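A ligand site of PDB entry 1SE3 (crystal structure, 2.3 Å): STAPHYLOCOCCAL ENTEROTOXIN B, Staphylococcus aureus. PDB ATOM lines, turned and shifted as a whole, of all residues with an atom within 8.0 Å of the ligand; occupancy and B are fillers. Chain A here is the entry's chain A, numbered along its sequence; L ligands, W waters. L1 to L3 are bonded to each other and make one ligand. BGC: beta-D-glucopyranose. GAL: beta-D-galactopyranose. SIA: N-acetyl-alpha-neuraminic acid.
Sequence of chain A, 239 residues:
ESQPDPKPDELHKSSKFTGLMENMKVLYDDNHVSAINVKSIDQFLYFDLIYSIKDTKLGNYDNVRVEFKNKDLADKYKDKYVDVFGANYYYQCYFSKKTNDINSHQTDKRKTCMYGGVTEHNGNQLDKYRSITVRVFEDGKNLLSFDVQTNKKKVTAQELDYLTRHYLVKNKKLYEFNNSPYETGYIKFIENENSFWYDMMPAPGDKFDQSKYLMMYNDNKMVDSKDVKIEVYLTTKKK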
ATOM      1  N   LYS A  39       4.459  -6.204  22.228  1.00  0.00           N
ATOM      2  CA  LYS A  39       3.593  -5.198  21.612  1.00  0.00           C
ATOM      3  C   LYS A  39       4.259  -4.713  20.335  1.00  0.00           C
ATOM      4  O   LYS A  39       5.471  -4.555  20.284  1.00  0.00           O
ATOM      5  CB  LYS A  39       3.420  -4.024  22.564  1.00  0.00           C
ATOM      6  CG  LYS A  39       2.407  -2.967  22.113  1.00  0.00           C
ATOM      7  CD  LYS A  39       2.696  -1.609  22.777  1.00  0.00           C
ATOM      8  CE  LYS A  39       3.799  -0.845  22.041  1.00  0.00           C
ATOM      9  NZ  LYS A  39       5.164  -1.479  22.091  1.00  0.00           N
ATOM     10  N   ILE A  41       6.000  -2.555  17.623  1.00  0.00           N
ATOM     11  CA  ILE A  41       6.825  -1.362  17.762  1.00  0.00           C
ATOM     12  C   ILE A  41       6.865  -0.477  16.532  1.00  0.00           C
ATOM     13  O   ILE A  41       7.367   0.642  16.596  1.00  0.00           O
ATOM     14  CB  ILE A  41       8.301  -1.708  18.067  1.00  0.00           C
ATOM     15  CG1 ILE A  41       8.824  -2.700  17.036  1.00  0.00           C
ATOM     16  CG2 ILE A  41       8.432  -2.252  19.443  1.00  0.00           C
ATOM     17  CD1 ILE A  41      10.295  -2.900  17.060  1.00  0.00           C
ATOM     18  N   ASP A  42       6.390  -0.989  15.384  1.00  0.00           N
ATOM     19  CA  ASP A  42       6.410  -0.271  14.114  1.00  0.00           C
ATOM     20  C   ASP A  42       5.435  -0.977  13.181  1.00  0.00           C
ATOM     21  O   ASP A  42       4.760  -1.923  13.582  1.00  0.00           O
ATOM     22  CB  ASP A  42       7.818  -0.296  13.515  1.00  0.00           C
ATOM     23  CG  ASP A  42       8.026   0.727  12.365  1.00  0.00           C
ATOM     24  OD1 ASP A  42       7.866   1.950  12.582  1.00  0.00           O
ATOM     25  OD2 ASP A  42       8.418   0.303  11.257  1.00  0.00           O
ATOM     26  N   ILE A  50       5.346  -4.765  13.065  1.00  0.00           N
ATOM     27  CA  ILE A  50       6.707  -5.177  13.277  1.00  0.00           C
ATOM     28  C   ILE A  50       6.890  -5.372  14.769  1.00  0.00           C
ATOM     29  O   ILE A  50       6.455  -4.542  15.563  1.00  0.00           O
ATOM     30  CB  ILE A  50       7.706  -4.140  12.763  1.00  0.00           C
ATOM     31  CG1 ILE A  50       7.393  -3.777  11.318  1.00  0.00           C
ATOM     32  CG2 ILE A  50       9.121  -4.652  12.895  1.00  0.00           C
ATOM     33  CD1 ILE A  50       7.351  -4.913  10.402  1.00  0.00           C
ATOM     34  N   TYR A  51       7.461  -6.522  15.137  1.00  0.00           N
ATOM     35  CA  TYR A  51       7.696  -6.854  16.530  1.00  0.00           C
ATOM     36  C   TYR A  51       9.168  -6.928  16.786  1.00  0.00           C
ATOM     37  O   TYR A  51       9.952  -7.229  15.890  1.00  0.00           O
ATOM     38  CB  TYR A  51       7.059  -8.188  16.901  1.00  0.00           C
ATOM     39  CG  TYR A  51       5.572  -8.119  17.081  1.00  0.00           C
ATOM     40  CD1 TYR A  51       5.011  -7.754  18.293  1.00  0.00           C
ATOM     41  CD2 TYR A  51       4.712  -8.349  16.012  1.00  0.00           C
ATOM     42  CE1 TYR A  51       3.641  -7.607  18.435  1.00  0.00           C
ATOM     43  CE2 TYR A  51       3.328  -8.198  16.147  1.00  0.00           C
ATOM     44  CZ  TYR A  51       2.809  -7.822  17.362  1.00  0.00           C
ATOM     45  OH  TYR A  51       1.463  -7.618  17.497  1.00  0.00           O
ATOM     46  N   SER A  52       9.541  -6.607  18.009  1.00  0.00           N
ATOM     47  CA  SER A  52      10.922  -6.687  18.446  1.00  0.00           C
ATOM     48  C   SER A  52      10.977  -8.058  19.123  1.00  0.00           C
ATOM     49  O   SER A  52      10.573  -8.214  20.271  1.00  0.00           O
ATOM     50  CB  SER A  52      11.199  -5.597  19.456  1.00  0.00           C
ATOM     51  OG  SER A  52      10.107  -4.682  19.461  1.00  0.00           O
ATOM     52  N   ILE A  53      11.323  -9.071  18.354  1.00  0.00           N
ATOM     53  CA  ILE A  53      11.435 -10.414  18.877  1.00  0.00           C
ATOM     54  C   ILE A  53      12.862 -10.816  18.566  1.00  0.00           C
ATOM     55  O   ILE A  53      13.387 -10.584  17.471  1.00  0.00           O
ATOM     56  CB  ILE A  53      10.364 -11.346  18.280  1.00  0.00           C
ATOM     57  CG1 ILE A  53       8.985 -10.812  18.669  1.00  0.00           C
ATOM     58  CG2 ILE A  53      10.552 -12.776  18.812  1.00  0.00           C
ATOM     59  CD1 ILE A  53       7.831 -11.574  18.125  1.00  0.00           C
ATOM     60  N   LYS A  54      13.529 -11.289  19.617  1.00  0.00           N
ATOM     61  CA  LYS A  54      14.919 -11.678  19.574  1.00  0.00           C
ATOM     62  C   LYS A  54      15.135 -13.169  19.488  1.00  0.00           C
ATOM     63  O   LYS A  54      14.597 -13.924  20.297  1.00  0.00           O
ATOM     64  CB  LYS A  54      15.584 -11.131  20.834  1.00  0.00           C
ATOM     65  CG  LYS A  54      17.000 -11.585  21.010  1.00  0.00           C
ATOM     66  CD  LYS A  54      17.698 -10.812  22.080  1.00  0.00           C
ATOM     67  CE  LYS A  54      19.131 -10.565  21.647  1.00  0.00           C
ATOM     68  NZ  LYS A  54      19.185  -9.869  20.317  1.00  0.00           N
ATOM     69  N   ASP A  55      15.930 -13.581  18.508  1.00  0.00           N
ATOM     70  CA  ASP A  55      16.228 -14.990  18.350  1.00  0.00           C
ATOM     71  C   ASP A  55      17.153 -15.323  19.494  1.00  0.00           C
ATOM     72  O   ASP A  55      18.387 -15.226  19.370  1.00  0.00           O
ATOM     73  CB  ASP A  55      16.946 -15.266  17.038  1.00  0.00           C
ATOM     74  CG  ASP A  55      17.202 -16.741  16.807  1.00  0.00           C
ATOM     75  OD1 ASP A  55      17.631 -17.444  17.738  1.00  0.00           O
ATOM     76  OD2 ASP A  55      16.983 -17.230  15.687  1.00  0.00           O
ATOM     77  N   TYR A  61      17.607 -13.443  14.198  1.00  0.00           N
ATOM     78  CA  TYR A  61      16.704 -12.318  14.022  1.00  0.00           C
ATOM     79  C   TYR A  61      16.558 -11.462  15.270  1.00  0.00           C
ATOM     80  O   TYR A  61      16.624 -11.958  16.401  1.00  0.00           O
ATOM     81  CB  TYR A  61      15.342 -12.793  13.515  1.00  0.00           C
ATOM     82  CG  TYR A  61      14.651 -13.807  14.388  1.00  0.00           C
ATOM     83  CD1 TYR A  61      13.916 -13.418  15.492  1.00  0.00           C
ATOM     84  CD2 TYR A  61      14.740 -15.168  14.092  1.00  0.00           C
ATOM     85  CE1 TYR A  61      13.287 -14.344  16.298  1.00  0.00           C
ATOM     86  CE2 TYR A  61      14.105 -16.113  14.907  1.00  0.00           C
ATOM     87  CZ  TYR A  61      13.386 -15.691  16.004  1.00  0.00           C
ATOM     88  OH  TYR A  61      12.757 -16.617  16.810  1.00  0.00           O
ATOM     89  N   ASP A  62      16.360 -10.173  15.012  1.00  0.00           N
ATOM     90  CA  ASP A  62      16.193  -9.138  16.027  1.00  0.00           C
ATOM     91  C   ASP A  62      14.802  -8.504  15.963  1.00  0.00           C
ATOM     92  O   ASP A  62      14.301  -8.005  16.978  1.00  0.00           O
ATOM     93  CB  ASP A  62      17.247  -8.061  15.806  1.00  0.00           C
ATOM     94  CG  ASP A  62      18.644  -8.587  15.972  1.00  0.00           C
ATOM     95  OD1 ASP A  62      18.871  -9.238  17.007  1.00  0.00           O
ATOM     96  OD2 ASP A  62      19.514  -8.368  15.101  1.00  0.00           O
ATOM     97  N   ASN A  63      14.197  -8.498  14.782  1.00  0.00           N
ATOM     98  CA  ASN A  63      12.860  -7.912  14.594  1.00  0.00           C
ATOM     99  C   ASN A  63      12.060  -8.940  13.807  1.00  0.00           C
ATOM    100  O   ASN A  63      12.653  -9.741  13.094  1.00  0.00           O
ATOM    101  CB  ASN A  63      12.967  -6.588  13.822  1.00  0.00           C
ATOM    102  CG  ASN A  63      13.725  -5.497  14.599  1.00  0.00           C
ATOM    103  OD1 ASN A  63      13.179  -4.898  15.522  1.00  0.00           O
ATOM    104  ND2 ASN A  63      14.969  -5.247  14.208  1.00  0.00           N
ATOM    105  N   GLN A 106      11.302   1.140  10.105  1.00  0.00           N
ATOM    106  CA  GLN A 106      12.072   0.938  11.329  1.00  0.00           C
ATOM    107  C   GLN A 106      12.891  -0.301  11.004  1.00  0.00           C
ATOM    108  O   GLN A 106      13.033  -0.667   9.847  1.00  0.00           O
ATOM    109  CB  GLN A 106      11.131   0.588  12.513  1.00  0.00           C
ATOM    110  CG  GLN A 106      11.705   0.674  13.974  1.00  0.00           C
ATOM    111  CD  GLN A 106      12.597  -0.510  14.414  1.00  0.00           C
ATOM    112  OE1 GLN A 106      13.806  -0.349  14.578  1.00  0.00           O
ATOM    113  NE2 GLN A 106      12.005  -1.693  14.519  1.00  0.00           N
ATOM    114  N   THR A 107      13.564  -0.789  12.037  1.00  0.00           N
ATOM    115  CA  THR A 107      14.306  -2.023  12.018  1.00  0.00           C
ATOM    116  C   THR A 107      15.771  -1.916  11.630  1.00  0.00           C
ATOM    117  O   THR A 107      16.096  -1.663  10.471  1.00  0.00           O
ATOM    118  CB  THR A 107      13.560  -3.046  11.177  1.00  0.00           C
ATOM    119  OG1 THR A 107      12.166  -3.045  11.554  1.00  0.00           O
ATOM    120  CG2 THR A 107      14.144  -4.430  11.407  1.00  0.00           C
ATOM    121  N   ASP A 108      16.641  -2.003  12.640  1.00  0.00           N
ATOM    122  CA  ASP A 108      18.075  -1.981  12.375  1.00  0.00           C
ATOM    123  C   ASP A 108      18.563  -3.441  12.668  1.00  0.00           C
ATOM    124  O   ASP A 108      18.279  -4.001  13.742  1.00  0.00           O
ATOM    125  CB  ASP A 108      18.875  -0.959  13.243  1.00  0.00           C
ATOM    126  CG  ASP A 108      18.307   0.477  13.236  1.00  0.00           C
ATOM    127  OD1 ASP A 108      17.524   0.830  12.328  1.00  0.00           O
ATOM    128  OD2 ASP A 108      18.689   1.275  14.133  1.00  0.00           O
ATOM    129  N   LYS A 109      19.128  -4.067  11.648  1.00  0.00           N
ATOM    130  CA  LYS A 109      19.664  -5.424  11.760  1.00  0.00           C
ATOM    131  C   LYS A 109      18.757  -6.654  11.901  1.00  0.00           C
ATOM    132  O   LYS A 109      17.819  -6.673  12.705  1.00  0.00           O
ATOM    133  CB  LYS A 109      20.742  -5.496  12.839  1.00  0.00           C
ATOM    134  CG  LYS A 109      21.428  -6.850  12.921  1.00  0.00           C
ATOM    135  CD  LYS A 109      22.792  -6.766  13.581  1.00  0.00           C
ATOM    136  CE  LYS A 109      23.653  -7.956  13.211  1.00  0.00           C
ATOM    137  NZ  LYS A 109      25.057  -7.731  13.677  1.00  0.00           N
ATOM    138  N   ARG A 110      19.100  -7.667  11.098  1.00  0.00           N
ATOM    139  CA  ARG A 110      18.473  -9.003  11.016  1.00  0.00           C
ATOM    140  C   ARG A 110      16.959  -9.185  11.033  1.00  0.00           C
ATOM    141  O   ARG A 110      16.330  -9.211  12.105  1.00  0.00           O
ATOM    142  CB  ARG A 110      19.157  -9.938  12.017  1.00  0.00           C
ATOM    143  CG  ARG A 110      20.646 -10.044  11.749  1.00  0.00           C
ATOM    144  CD  ARG A 110      21.327 -11.059  12.636  1.00  0.00           C
ATOM    145  NE  ARG A 110      22.705 -11.256  12.194  1.00  0.00           N
ATOM    146  CZ  ARG A 110      23.737 -11.514  12.990  1.00  0.00           C
ATOM    147  NH1 ARG A 110      23.555 -11.619  14.312  1.00  0.00           N
ATOM    148  NH2 ARG A 110      24.946 -11.661  12.485  1.00  0.00           N
HETATM  149  C2  BGC L   1      24.678  -2.465  22.659  1.00  0.00           C
HETATM  150  C3  BGC L   1      23.881  -1.437  21.863  1.00  0.00           C
HETATM  151  C4  BGC L   1      22.380  -1.599  22.172  1.00  0.00           C
HETATM  152  C5  BGC L   1      22.070  -1.692  23.692  1.00  0.00           C
HETATM  153  C6  BGC L   1      20.672  -2.282  23.931  1.00  0.00           C
HETATM  154  C1  BGC L   1      24.377  -2.268  24.140  1.00  0.00           C
HETATM  155  O1  BGC L   1      25.167  -3.126  24.905  1.00  0.00           O
HETATM  156  O2  BGC L   1      26.068  -2.302  22.398  1.00  0.00           O
HETATM  157  O3  BGC L   1      24.133  -1.611  20.457  1.00  0.00           O
HETATM  158  O4  BGC L   1      21.675  -0.462  21.618  1.00  0.00           O
HETATM  159  O5  BGC L   1      22.998  -2.583  24.389  1.00  0.00           O
HETATM  160  O6  BGC L   1      20.691  -3.710  23.911  1.00  0.00           O
HETATM  161  C1  GAL L   2      21.427  -0.531  20.253  1.00  0.00           C
HETATM  162  C2  GAL L   2      20.120  -1.259  19.962  1.00  0.00           C
HETATM  163  C3  GAL L   2      20.013  -1.386  18.447  1.00  0.00           C
HETATM  164  C4  GAL L   2      19.981   0.025  17.812  1.00  0.00           C
HETATM  165  C5  GAL L   2      21.243   0.808  18.278  1.00  0.00           C
HETATM  166  C6  GAL L   2      21.293   2.269  17.844  1.00  0.00           C
HETATM  167  O2  GAL L   2      20.070  -2.532  20.615  1.00  0.00           O
HETATM  168  O3  GAL L   2      18.808  -2.138  18.107  1.00  0.00           O
HETATM  169  O4  GAL L   2      18.793   0.712  18.177  1.00  0.00           O
HETATM  170  O5  GAL L   2      21.357   0.797  19.721  1.00  0.00           O
HETATM  171  O6  GAL L   2      22.452   2.895  18.395  1.00  0.00           O
HETATM  172  C1  SIA L   3      20.184  -2.989  16.310  1.00  0.00           C
HETATM  173  C2  SIA L   3      18.753  -2.826  16.885  1.00  0.00           C
HETATM  174  C3  SIA L   3      17.832  -2.083  15.917  1.00  0.00           C
HETATM  175  C4  SIA L   3      16.364  -2.366  16.195  1.00  0.00           C
HETATM  176  C5  SIA L   3      16.224  -2.867  17.658  1.00  0.00           C
HETATM  177  C6  SIA L   3      16.961  -4.217  17.789  1.00  0.00           C
HETATM  178  C7  SIA L   3      17.137  -4.775  19.222  1.00  0.00           C
HETATM  179  C8  SIA L   3      17.958  -6.077  19.136  1.00  0.00           C
HETATM  180  C9  SIA L   3      18.348  -6.604  20.518  1.00  0.00           C
HETATM  181  C10 SIA L   3      14.388  -2.600  19.223  1.00  0.00           C
HETATM  182  C11 SIA L   3      12.902  -2.786  19.480  1.00  0.00           C
HETATM  183  N5  SIA L   3      14.819  -3.001  18.025  1.00  0.00           N
HETATM  184  O1A SIA L   3      20.644  -2.080  15.535  1.00  0.00           O
HETATM  185  O1B SIA L   3      20.882  -3.967  16.691  1.00  0.00           O
HETATM  186  O4  SIA L   3      15.591  -1.183  16.007  1.00  0.00           O
HETATM  187  O6  SIA L   3      18.256  -4.174  17.112  1.00  0.00           O
HETATM  188  O7  SIA L   3      17.794  -3.828  20.091  1.00  0.00           O
HETATM  189  O8  SIA L   3      17.208  -7.081  18.458  1.00  0.00           O
HETATM  190  O9  SIA L   3      17.334  -7.489  20.977  1.00  0.00           O
HETATM  191  O10 SIA L   3      15.140  -2.159  20.122  1.00  0.00           O
HETATM  192  O   HOH W   1      20.800  -4.865  21.675  1.00  0.00           O
HETATM  193  O   HOH W   2      26.282  -0.454  17.954  1.00  0.00           O
HETATM  194  O   HOH W   3      20.266  -7.211  23.109  1.00  0.00           O
HETATM  195  O   HOH W   4      23.688  -4.310  27.493  1.00  0.00           O
HETATM  196  O   HOH W   5      22.574  -3.155  13.691  1.00  0.00           O
HETATM  197  O   HOH W   6      23.454  -2.693  18.092  1.00  0.00           O
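OG1 of Thr 107 sits close to NE2 of Gln 106 (3.3 Å).
The backbone NH (N) of Gln 106 sits close to the side-chain carboxylate (OD2) of Asp 42.
NZ of Lys 54 lies within salt-bridge range of OD1 of Asp 62, 3.4 Å away.
The backbone NH of Ile 53 is in hydrogen-bond range of the backbone carbonyl oxygen of Asp 62.
The backbone NH (N) of Asp 62 sits at hydrogen-bond distance from the backbone carbonyl oxygen (O) of Arg 110, at 3.1 Å.
The backbone NH of Asn 63 is in hydrogen-bond range of the backbone carbonyl oxygen of Ile 53, at 3.5 Å.
The backbone NH of Asn 63 lies within hydrogen-bond range of the backbone carbonyl oxygen of Arg 110 (3.5 Å).
O of Ile 50 sits at hydrogen-bond distance from N of Ile 41.
The side-chain amide oxygen (OE1) of Gln 106 sits at hydrogen-bond distance from an oxygen (O4) of SIA L3, at 2.4 Å.
O of Asp 62 lies close to O8 of SIA L3.
OD1 of Asp 62 lies close to O8 of SIA L3 (3.1 Å).
The side-chain amino group of Lys 54 sits at hydrogen-bond distance from an oxygen (O9) of SIA L3, 3.1 Å away.
O of Asp 108 sits close to O6 of SIA L3.
Residues that only touch the ligand: Ser 52 (3.3 Å), Asn 63 (3.5 Å) and Ile 41 (3.6 Å).
Within 4 Å of the ligand: Ile 41, Ser 52, Lys 54, Asp 62, Asn 63, Gln 106 and Asp 108.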
